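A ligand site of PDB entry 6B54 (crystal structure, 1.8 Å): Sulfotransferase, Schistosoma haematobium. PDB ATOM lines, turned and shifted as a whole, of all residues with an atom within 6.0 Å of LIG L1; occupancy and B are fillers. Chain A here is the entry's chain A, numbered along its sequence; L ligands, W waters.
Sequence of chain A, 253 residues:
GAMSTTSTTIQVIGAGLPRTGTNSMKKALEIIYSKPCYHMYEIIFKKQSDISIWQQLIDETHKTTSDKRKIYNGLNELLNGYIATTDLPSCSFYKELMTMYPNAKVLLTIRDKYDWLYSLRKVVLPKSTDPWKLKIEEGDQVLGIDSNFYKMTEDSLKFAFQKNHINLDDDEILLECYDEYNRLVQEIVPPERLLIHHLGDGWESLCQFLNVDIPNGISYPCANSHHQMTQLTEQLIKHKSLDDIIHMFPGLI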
ATOM      1  N   LEU A  17     -12.201  23.318  -4.215  1.00  0.00           N
ATOM      2  CA  LEU A  17     -12.174  24.590  -4.928  1.00  0.00           C
ATOM      3  C   LEU A  17     -11.979  24.421  -6.442  1.00  0.00           C
ATOM      4  O   LEU A  17     -11.530  23.360  -6.910  1.00  0.00           O
ATOM      5  CB  LEU A  17     -11.052  25.467  -4.330  1.00  0.00           C
ATOM      6  CG  LEU A  17     -11.355  25.942  -2.905  1.00  0.00           C
ATOM      7  CD1 LEU A  17     -10.068  26.488  -2.267  1.00  0.00           C
ATOM      8  CD2 LEU A  17     -12.436  27.004  -2.934  1.00  0.00           C
ATOM      9  N   PRO A  18     -12.318  25.463  -7.236  1.00  0.00           N
ATOM     10  CA  PRO A  18     -12.032  25.364  -8.671  1.00  0.00           C
ATOM     11  C   PRO A  18     -10.559  25.126  -8.920  1.00  0.00           C
ATOM     12  O   PRO A  18      -9.732  25.557  -8.099  1.00  0.00           O
ATOM     13  CB  PRO A  18     -12.452  26.738  -9.230  1.00  0.00           C
ATOM     14  CG  PRO A  18     -12.455  27.647  -8.049  1.00  0.00           C
ATOM     15  CD  PRO A  18     -12.893  26.774  -6.882  1.00  0.00           C
ATOM     16  N   ARG A  19     -10.261  24.483 -10.036  1.00  0.00           N
ATOM     17  CA  ARG A  19      -8.907  24.095 -10.451  1.00  0.00           C
ATOM     18  C   ARG A  19      -8.234  23.069  -9.555  1.00  0.00           C
ATOM     19  O   ARG A  19      -7.015  23.007  -9.522  1.00  0.00           O
ATOM     20  CB  ARG A  19      -8.002  25.323 -10.582  1.00  0.00           C
ATOM     21  CG  ARG A  19      -8.595  26.438 -11.442  1.00  0.00           C
ATOM     22  CD  ARG A  19      -9.174  25.921 -12.756  1.00  0.00           C
ATOM     23  NE  ARG A  19      -8.174  25.397 -13.668  1.00  0.00           N
ATOM     24  CZ  ARG A  19      -8.451  24.859 -14.842  1.00  0.00           C
ATOM     25  NH1 ARG A  19      -9.726  24.757 -15.240  1.00  0.00           N
ATOM     26  NH2 ARG A  19      -7.474  24.404 -15.616  1.00  0.00           N
ATOM     27  N   THR A  20      -9.016  22.231  -8.869  1.00  0.00           N
ATOM     28  CA  THR A  20      -8.482  21.107  -8.122  1.00  0.00           C
ATOM     29  C   THR A  20      -8.888  19.744  -8.682  1.00  0.00           C
ATOM     30  O   THR A  20      -8.856  18.739  -7.951  1.00  0.00           O
ATOM     31  CB  THR A  20      -8.921  21.154  -6.632  1.00  0.00           C
ATOM     32  OG1 THR A  20     -10.357  21.064  -6.569  1.00  0.00           O
ATOM     33  CG2 THR A  20      -8.454  22.420  -5.961  1.00  0.00           C
ATOM     34  N   GLY A  21      -9.284  19.687  -9.949  1.00  0.00           N
ATOM     35  CA  GLY A  21      -9.689  18.434 -10.544  1.00  0.00           C
ATOM     36  C   GLY A  21     -11.196  18.187 -10.512  1.00  0.00           C
ATOM     37  O   GLY A  21     -11.650  17.037 -10.568  1.00  0.00           O
ATOM     38  N   THR A  22     -11.980  19.259 -10.446  1.00  0.00           N
ATOM     39  CA  THR A  22     -13.425  19.094 -10.271  1.00  0.00           C
ATOM     40  C   THR A  22     -14.120  18.594 -11.528  1.00  0.00           C
ATOM     41  O   THR A  22     -15.093  17.841 -11.419  1.00  0.00           O
ATOM     42  CB  THR A  22     -14.105  20.403  -9.817  1.00  0.00           C
ATOM     43  OG1 THR A  22     -13.840  21.428 -10.778  1.00  0.00           O
ATOM     44  CG2 THR A  22     -13.530  20.830  -8.440  1.00  0.00           C
ATOM     45  N   ASN A  23     -13.638  19.011 -12.708  1.00  0.00           N
ATOM     46  CA  ASN A  23     -14.283  18.542 -13.946  1.00  0.00           C
ATOM     47  C   ASN A  23     -14.026  17.041 -14.142  1.00  0.00           C
ATOM     48  O   ASN A  23     -14.927  16.293 -14.559  1.00  0.00           O
ATOM     49  CB  ASN A  23     -13.813  19.321 -15.185  1.00  0.00           C
ATOM     50  CG  ASN A  23     -14.649  18.985 -16.416  1.00  0.00           C
ATOM     51  OD1 ASN A  23     -14.231  18.194 -17.262  1.00  0.00           O
ATOM     52  ND2 ASN A  23     -15.851  19.554 -16.503  1.00  0.00           N
ATOM     53  N   SER A  24     -12.817  16.583 -13.793  1.00  0.00           N
ATOM     54  CA  SER A  24     -12.532  15.144 -13.809  1.00  0.00           C
ATOM     55  C   SER A  24     -13.397  14.398 -12.781  1.00  0.00           C
ATOM     56  O   SER A  24     -13.920  13.300 -13.066  1.00  0.00           O
ATOM     57  CB  SER A  24     -11.037  14.906 -13.540  1.00  0.00           C
ATOM     58  OG  SER A  24     -10.258  15.330 -14.667  1.00  0.00           O
ATOM     59  N   HIS A  39     -21.487  21.334 -12.200  1.00  0.00           N
ATOM     60  CA  HIS A  39     -20.112  21.840 -12.382  1.00  0.00           C
ATOM     61  C   HIS A  39     -20.256  23.198 -13.035  1.00  0.00           C
ATOM     62  O   HIS A  39     -21.309  23.512 -13.590  1.00  0.00           O
ATOM     63  CB  HIS A  39     -19.266  20.893 -13.272  1.00  0.00           C
ATOM     64  CG  HIS A  39     -17.800  21.255 -13.340  1.00  0.00           C
ATOM     65  ND1 HIS A  39     -17.272  22.069 -14.326  1.00  0.00           N
ATOM     66  CD2 HIS A  39     -16.763  20.920 -12.528  1.00  0.00           C
ATOM     67  CE1 HIS A  39     -15.970  22.216 -14.123  1.00  0.00           C
ATOM     68  NE2 HIS A  39     -15.640  21.534 -13.041  1.00  0.00           N
ATOM     69  N   ASP A  87     -17.246  21.992  -7.930  1.00  0.00           N
ATOM     70  CA  ASP A  87     -16.753  23.254  -8.492  1.00  0.00           C
ATOM     71  C   ASP A  87     -17.435  24.479  -7.890  1.00  0.00           C
ATOM     72  O   ASP A  87     -18.430  24.381  -7.150  1.00  0.00           O
ATOM     73  CB  ASP A  87     -16.929  23.239 -10.019  1.00  0.00           C
ATOM     74  CG  ASP A  87     -16.012  24.202 -10.764  1.00  0.00           C
ATOM     75  OD1 ASP A  87     -15.157  24.893 -10.145  1.00  0.00           O
ATOM     76  OD2 ASP A  87     -16.142  24.223 -12.005  1.00  0.00           O
ATOM     77  N   ARG A 111      -4.908  19.675  -4.192  1.00  0.00           N
ATOM     78  CA  ARG A 111      -3.675  19.581  -4.964  1.00  0.00           C
ATOM     79  C   ARG A 111      -2.666  20.543  -4.350  1.00  0.00           C
ATOM     80  O   ARG A 111      -3.022  21.389  -3.515  1.00  0.00           O
ATOM     81  CB  ARG A 111      -3.901  19.925  -6.436  1.00  0.00           C
ATOM     82  CG  ARG A 111      -4.037  21.445  -6.654  1.00  0.00           C
ATOM     83  CD  ARG A 111      -4.429  21.799  -8.083  1.00  0.00           C
ATOM     84  NE  ARG A 111      -3.365  21.524  -9.054  1.00  0.00           N
ATOM     85  CZ  ARG A 111      -3.439  21.864 -10.344  1.00  0.00           C
ATOM     86  NH1 ARG A 111      -4.502  22.509 -10.820  1.00  0.00           N
ATOM     87  NH2 ARG A 111      -2.435  21.567 -11.171  1.00  0.00           N
ATOM     88  N   ASP A 115       0.601  25.025  -7.601  1.00  0.00           N
ATOM     89  CA  ASP A 115       0.040  24.629  -8.894  1.00  0.00           C
ATOM     90  C   ASP A 115      -1.409  25.133  -9.018  1.00  0.00           C
ATOM     91  O   ASP A 115      -1.834  25.569 -10.076  1.00  0.00           O
ATOM     92  CB  ASP A 115       0.056  23.119  -9.080  1.00  0.00           C
ATOM     93  CG  ASP A 115       1.461  22.541  -9.207  1.00  0.00           C
ATOM     94  OD1 ASP A 115       2.414  23.291  -9.513  1.00  0.00           O
ATOM     95  OD2 ASP A 115       1.566  21.305  -9.036  1.00  0.00           O
ATOM     96  N   SER A 119      -2.921  27.708 -11.797  1.00  0.00           N
ATOM     97  CA  SER A 119      -4.077  27.298 -12.594  1.00  0.00           C
ATOM     98  C   SER A 119      -5.197  28.335 -12.472  1.00  0.00           C
ATOM     99  O   SER A 119      -5.813  28.731 -13.483  1.00  0.00           O
ATOM    100  CB  SER A 119      -4.540  25.916 -12.153  1.00  0.00           C
ATOM    101  OG  SER A 119      -5.454  25.378 -13.093  1.00  0.00           O
ATOM    102  N   VAL A 123      -7.251  30.787 -15.578  1.00  0.00           N
ATOM    103  CA  VAL A 123      -8.595  30.420 -16.036  1.00  0.00           C
ATOM    104  C   VAL A 123      -9.697  31.193 -15.323  1.00  0.00           C
ATOM    105  O   VAL A 123     -10.585  31.734 -15.965  1.00  0.00           O
ATOM    106  CB  VAL A 123      -8.833  28.916 -15.872  1.00  0.00           C
ATOM    107  CG1 VAL A 123     -10.249  28.541 -16.315  1.00  0.00           C
ATOM    108  CG2 VAL A 123      -7.793  28.107 -16.667  1.00  0.00           C
ATOM    109  N   LEU A 199      -5.028  15.122  -6.348  1.00  0.00           N
ATOM    110  CA  LEU A 199      -4.825  15.059  -7.777  1.00  0.00           C
ATOM    111  C   LEU A 199      -3.937  13.851  -8.077  1.00  0.00           C
ATOM    112  O   LEU A 199      -2.904  13.674  -7.439  1.00  0.00           O
ATOM    113  CB  LEU A 199      -4.182  16.351  -8.265  1.00  0.00           C
ATOM    114  CG  LEU A 199      -4.593  16.887  -9.627  1.00  0.00           C
ATOM    115  CD1 LEU A 199      -6.103  16.885  -9.781  1.00  0.00           C
ATOM    116  CD2 LEU A 199      -4.019  18.278  -9.801  1.00  0.00           C
ATOM    117  N   GLY A 200      -4.370  13.005  -9.010  1.00  0.00           N
ATOM    118  CA  GLY A 200      -3.652  11.776  -9.293  1.00  0.00           C
ATOM    119  C   GLY A 200      -4.180  10.517  -8.596  1.00  0.00           C
ATOM    120  O   GLY A 200      -3.819   9.419  -9.011  1.00  0.00           O
ATOM    121  N   TYR A 220      -9.464   6.710 -15.146  1.00  0.00           N
ATOM    122  CA  TYR A 220      -9.933   7.874 -14.380  1.00  0.00           C
ATOM    123  C   TYR A 220      -9.815   9.120 -15.248  1.00  0.00           C
ATOM    124  O   TYR A 220      -8.801   9.302 -15.902  1.00  0.00           O
ATOM    125  CB  TYR A 220      -9.138   8.028 -13.081  1.00  0.00           C
ATOM    126  CG  TYR A 220      -9.762   9.096 -12.229  1.00  0.00           C
ATOM    127  CD1 TYR A 220     -10.814   8.805 -11.370  1.00  0.00           C
ATOM    128  CD2 TYR A 220      -9.329  10.415 -12.319  1.00  0.00           C
ATOM    129  CE1 TYR A 220     -11.409   9.794 -10.605  1.00  0.00           C
ATOM    130  CE2 TYR A 220      -9.920  11.410 -11.562  1.00  0.00           C
ATOM    131  CZ  TYR A 220     -10.971  11.101 -10.716  1.00  0.00           C
ATOM    132  OH  TYR A 220     -11.545  12.088  -9.958  1.00  0.00           O
ATOM    133  N   PRO A 221     -10.856   9.977 -15.271  1.00  0.00           N
ATOM    134  CA  PRO A 221     -10.821  11.100 -16.216  1.00  0.00           C
ATOM    135  C   PRO A 221      -9.674  12.053 -15.950  1.00  0.00           C
ATOM    136  O   PRO A 221      -9.222  12.193 -14.794  1.00  0.00           O
ATOM    137  CB  PRO A 221     -12.166  11.797 -16.013  1.00  0.00           C
ATOM    138  CG  PRO A 221     -13.077  10.708 -15.430  1.00  0.00           C
ATOM    139  CD  PRO A 221     -12.147   9.913 -14.552  1.00  0.00           C
ATOM    140  N   CYS A 222      -9.208  12.702 -17.010  1.00  0.00           N
ATOM    141  CA  CYS A 222      -8.145  13.704 -16.902  1.00  0.00           C
ATOM    142  C   CYS A 222      -8.448  14.852 -17.852  1.00  0.00           C
ATOM    143  O   CYS A 222      -8.020  14.820 -18.988  1.00  0.00           O
ATOM    144  CB  CYS A 222      -6.786  13.072 -17.223  1.00  0.00           C
ATOM    145  SG  CYS A 222      -5.389  14.141 -16.853  1.00  0.00           S
ATOM    146  N   ALA A 223      -9.201  15.849 -17.376  1.00  0.00           N
ATOM    147  CA  ALA A 223      -9.734  16.884 -18.246  1.00  0.00           C
ATOM    148  C   ALA A 223      -9.502  18.281 -17.693  1.00  0.00           C
ATOM    149  O   ALA A 223      -9.251  18.425 -16.501  1.00  0.00           O
ATOM    150  CB  ALA A 223     -11.240  16.653 -18.441  1.00  0.00           C
ATOM    151  N   ASN A 224      -9.607  19.291 -18.573  1.00  0.00           N
ATOM    152  CA  ASN A 224      -9.756  20.688 -18.144  1.00  0.00           C
ATOM    153  C   ASN A 224      -8.423  21.294 -17.666  1.00  0.00           C
ATOM    154  O   ASN A 224      -8.387  22.011 -16.643  1.00  0.00           O
ATOM    155  CB  ASN A 224     -10.826  20.784 -17.033  1.00  0.00           C
ATOM    156  CG  ASN A 224     -11.378  22.175 -16.848  1.00  0.00           C
ATOM    157  OD1 ASN A 224     -11.310  23.020 -17.740  1.00  0.00           O
ATOM    158  ND2 ASN A 224     -11.901  22.437 -15.655  1.00  0.00           N
ATOM    159  N   SER A 225      -7.345  21.013 -18.396  1.00  0.00           N
ATOM    160  CA  SER A 225      -6.019  21.616 -18.123  1.00  0.00           C
ATOM    161  C   SER A 225      -6.015  23.120 -18.440  1.00  0.00           C
ATOM    162  O   SER A 225      -6.785  23.553 -19.289  1.00  0.00           O
ATOM    163  CB  SER A 225      -4.945  20.915 -18.940  1.00  0.00           C
ATOM    164  OG  SER A 225      -5.050  21.323 -20.297  1.00  0.00           O
ATOM    165  N   HIS A 226      -5.146  23.924 -17.821  1.00  0.00           N
ATOM    166  CA  HIS A 226      -5.140  25.341 -18.218  1.00  0.00           C
ATOM    167  C   HIS A 226      -4.593  25.481 -19.650  1.00  0.00           C
ATOM    168  O   HIS A 226      -4.896  26.448 -20.340  1.00  0.00           O
ATOM    169  CB  HIS A 226      -4.372  26.249 -17.214  1.00  0.00           C
ATOM    170  CG  HIS A 226      -2.911  25.962 -17.091  1.00  0.00           C
ATOM    171  ND1 HIS A 226      -1.975  26.416 -17.995  1.00  0.00           N
ATOM    172  CD2 HIS A 226      -2.209  25.318 -16.114  1.00  0.00           C
ATOM    173  CE1 HIS A 226      -0.769  26.042 -17.608  1.00  0.00           C
ATOM    174  NE2 HIS A 226      -0.879  25.363 -16.472  1.00  0.00           N
ATOM    175  N   HIS A 227      -3.855  24.477 -20.110  1.00  0.00           N
ATOM    176  CA  HIS A 227      -3.361  24.497 -21.498  1.00  0.00           C
ATOM    177  C   HIS A 227      -4.527  24.384 -22.471  1.00  0.00           C
ATOM    178  O   HIS A 227      -4.570  25.055 -23.491  1.00  0.00           O
ATOM    179  CB  HIS A 227      -2.377  23.346 -21.753  1.00  0.00           C
ATOM    180  CG  HIS A 227      -1.167  23.389 -20.869  1.00  0.00           C
ATOM    181  ND1 HIS A 227      -0.396  24.523 -20.717  1.00  0.00           N
ATOM    182  CD2 HIS A 227      -0.586  22.442 -20.098  1.00  0.00           C
ATOM    183  CE1 HIS A 227       0.605  24.273 -19.882  1.00  0.00           C
ATOM    184  NE2 HIS A 227       0.503  23.017 -19.495  1.00  0.00           N
HETATM  185  P1  LIG L   1      -3.919  22.492 -14.454  1.00  0.00           P
HETATM  186  O1  LIG L   1      -3.580  21.745 -15.713  1.00  0.00           O
HETATM  187  O2  LIG L   1      -2.699  22.767 -13.613  1.00  0.00           O
HETATM  188  O3  LIG L   1      -4.605  23.798 -14.765  1.00  0.00           O
HETATM  189  P2  LIG L   1     -10.856  21.861 -12.397  1.00  0.00           P
HETATM  190  O4  LIG L   1     -11.606  20.923 -13.349  1.00  0.00           O
HETATM  191  O5  LIG L   1     -11.431  21.900 -11.012  1.00  0.00           O
HETATM  192  O6  LIG L   1     -10.815  23.224 -13.074  1.00  0.00           O
HETATM  193  O7  LIG L   1      -9.387  21.243 -12.260  1.00  0.00           O
HETATM  194  C1  LIG L   1      -8.525  21.351 -13.395  1.00  0.00           C
HETATM  195  C2  LIG L   1      -7.119  20.993 -12.991  1.00  0.00           C
HETATM  196  O8  LIG L   1      -6.996  19.609 -12.527  1.00  0.00           O
HETATM  197  C3  LIG L   1      -6.130  21.107 -14.121  1.00  0.00           C
HETATM  198  O9  LIG L   1      -4.876  21.544 -13.567  1.00  0.00           O
HETATM  199  C4  LIG L   1      -6.087  19.720 -14.641  1.00  0.00           C
HETATM  200  O10 LIG L   1      -4.941  19.502 -15.440  1.00  0.00           O
HETATM  201  C5  LIG L   1      -6.044  18.931 -13.365  1.00  0.00           C
HETATM  202  N1  LIG L   1      -6.468  17.576 -13.499  1.00  0.00           N
HETATM  203  C6  LIG L   1      -7.700  17.129 -13.797  1.00  0.00           C
HETATM  204  N2  LIG L   1      -7.706  15.780 -13.802  1.00  0.00           N
HETATM  205  C7  LIG L   1      -6.440  15.344 -13.504  1.00  0.00           C
HETATM  206  C8  LIG L   1      -5.808  14.056 -13.336  1.00  0.00           C
HETATM  207  N3  LIG L   1      -6.536  12.873 -13.521  1.00  0.00           N
HETATM  208  N4  LIG L   1      -4.498  14.007 -13.013  1.00  0.00           N
HETATM  209  C9  LIG L   1      -3.785  15.117 -12.838  1.00  0.00           C
HETATM  210  N5  LIG L   1      -4.332  16.332 -12.960  1.00  0.00           N
HETATM  211  C10 LIG L   1      -5.644  16.486 -13.282  1.00  0.00           C
HETATM  212  C1  LG2 L   2     -14.325  27.195 -15.015  1.00  0.00           C
HETATM  213  C2  LG2 L   2     -14.483  28.043 -13.906  1.00  0.00           C
HETATM  214  C3  LG2 L   2     -14.516  29.437 -14.138  1.00  0.00           C
HETATM  215  C4  LG2 L   2     -14.393  29.939 -15.418  1.00  0.00           C
HETATM  216  C5  LG2 L   2     -14.235  29.092 -16.499  1.00  0.00           C
HETATM  217  C6  LG2 L   2     -14.199  27.701 -16.318  1.00  0.00           C
HETATM  218  C7  LG2 L   2     -13.818  28.853 -18.947  1.00  0.00           C
HETATM  219  C8  LG2 L   2     -14.500  27.471 -18.773  1.00  0.00           C
HETATM  220  C9  LG2 L   2     -14.037  26.819 -17.424  1.00  0.00           C
HETATM  221  C10 LG2 L   2     -14.582  27.456 -12.641  1.00  0.00           C
HETATM  222  C11 LG2 L   2     -14.263  29.564 -20.228  1.00  0.00           C
HETATM  223  C12 LG2 L   2     -13.677  30.827 -22.832  1.00  0.00           C
HETATM  224  C13 LG2 L   2     -11.826  29.603 -21.745  1.00  0.00           C
HETATM  225  C14 LG2 L   2     -12.744  30.829 -21.630  1.00  0.00           C
HETATM  226  N1  LG2 L   2     -14.124  29.680 -17.771  1.00  0.00           N
HETATM  227  N2  LG2 L   2     -14.680  30.351 -13.182  1.00  0.00           N
HETATM  228  N3  LG2 L   2     -13.521  30.845 -20.376  1.00  0.00           N
HETATM  229  O1  LG2 L   2     -14.516  31.598 -13.561  1.00  0.00           O
HETATM  230  O2  LG2 L   2     -15.041  30.068 -11.806  1.00  0.00           O
HETATM  231  O3  LG2 L   2     -14.480  26.048 -12.792  1.00  0.00           O
HETATM  232  O   HOH W   1      -4.806  17.246 -17.166  1.00  0.00           O
HETATM  233  O   HOH W   2      -1.903  18.153 -13.316  1.00  0.00           O
HETATM  234  O   HOH W   3     -10.580  18.396 -13.863  1.00  0.00           O
HETATM  235  O   HOH W   4      -0.989  24.612 -12.603  1.00  0.00           O
HETATM  236  O   HOH W   5      -5.653  10.001 -12.721  1.00  0.00           O
HETATM  237  O   HOH W   6      -0.710  20.527 -14.120  1.00  0.00           O
HETATM  238  O   HOH W   7     -12.458  24.725 -14.004  1.00  0.00           O
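OG of Ser 119 lies within hydrogen-bond range of O3 of LIG L1 (2.5 Å).
The backbone NH (N) of Thr 22 lies within hydrogen-bond range of an oxygen (O5) of LIG L1.
The side-chain hydroxyl (OG1) of Thr 22 is in hydrogen-bond range of an oxygen (O5) of LIG L1 (2.5 Å).
The side-chain hydroxyl (OG) of Ser 24 sits at hydrogen-bond distance from a nitrogen (N2) of LIG L1, 2.7 Å away.
NH2 of Arg 111 lies within salt-bridge range of O2 of LIG L1, 2.7 Å away.
ND2 of Asn 224 lies within hydrogen-bond range of O4 of LIG L1, 2.8 Å away.
The backbone NH of Gly 21 sits at hydrogen-bond distance from an oxygen (O7) of LIG L1, 2.8 Å away.
O4 of LIG L1 is in hydrogen-bond range of N of Asn 23 (2.9 Å).
O5 of LIG L1 lies within hydrogen-bond range of N of Arg 19 (3.0 Å).
NH1 of Arg 19 lies within salt-bridge range of O6 of LIG L1 (2.9 Å).
O of Pro 221 sits at hydrogen-bond distance from N3 of LIG L1 (3.0 Å).
N of His 226 lies within hydrogen-bond range of O3 of LIG L1 (3.1 Å).
The backbone NH of Thr 20 lies within hydrogen-bond range of an oxygen (O5) of LIG L1, 3.2 Å away.
N3 of LIG L1 lies close to SG of Cys 222.
The side-chain carboxylate (OD2) of Asp 87 sits at hydrogen-bond distance from an oxygen (O3) of LG2 L2, at 2.6 Å.
NE of Arg 19 lies within hydrogen-bond range of OG of Ser 119 (2.8 Å).
The side-chain hydroxyl (OG1) of Thr 22 sits at hydrogen-bond distance from a ring nitrogen (NE2) of His 39, at 2.9 Å.
The side-chain hydroxyl (OG) of Ser 24 is in hydrogen-bond range of the backbone carbonyl oxygen (O) of Pro 221, at 3.3 Å.
NH1 of Arg 111 sits at hydrogen-bond distance from O of Arg 19 (2.9 Å).
O of Asn 224 is in hydrogen-bond range of NH2 of Arg 19 (2.8 Å).
A ring nitrogen (NE2) of His 39 sits at hydrogen-bond distance from the backbone NH of Asn 23, at 3.2 Å.
O of Leu 17 lies within hydrogen-bond range of OG1 of Thr 20.
The side-chain hydroxyl (OG) of Ser 225 lies close to the backbone NH (N) of His 227 (3.4 Å).
C of Pro 18 touches O5 of LIG L1, at 3.9 Å.
Leu 199 touches LIG L1.
CD2 of Tyr 220 touches N3 of LIG L1, 3.9 Å away.
Ala 223 touches LIG L1.
Ser 225 touches LIG L1.
Hydrophobic or aromatic side chains that line LIG L1: Leu 199, Tyr 220 and His 226.
Within 4 Å of LIG L1: Pro 18, Arg 19, Thr 20, Gly 21, Thr 22, Asn 23, Ser 24, Arg 111, Ser 119, Leu 199, Tyr 220, Pro 221, Cys 222, Ala 223, Asn 224, Ser 225 and His 226.
Along chain A the residues within 4 Å of LIG L1 span positions 18 to 226.
The nearest printed residue that does not touch LIG L1 is His 39 (4.1 Å).
Water W7 lies within hydrogen-bond range of O6 of LIG L1 (2.4 Å), O3 of LG2 L2 (2.7 Å), ND2 of Asn 224 (2.9 Å) and NH1 of Arg 19 (3.0 Å).
Water W4 bridges O2 of LIG L1 and O of Asp 115.
Water W3 lies within hydrogen-bond range of an oxygen (O4) of LIG L1 (2.8 Å), the backbone NH of Ser 24 (2.9 Å), the backbone carbonyl oxygen of Ala 223 (3.0 Å) and the backbone NH of Asn 23 (3.3 Å).
Water W1 lies within hydrogen-bond range of an oxygen (O10) of LIG L1 (2.8 Å) and the side-chain sulfur (SG) of Cys 222 (3.2 Å).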
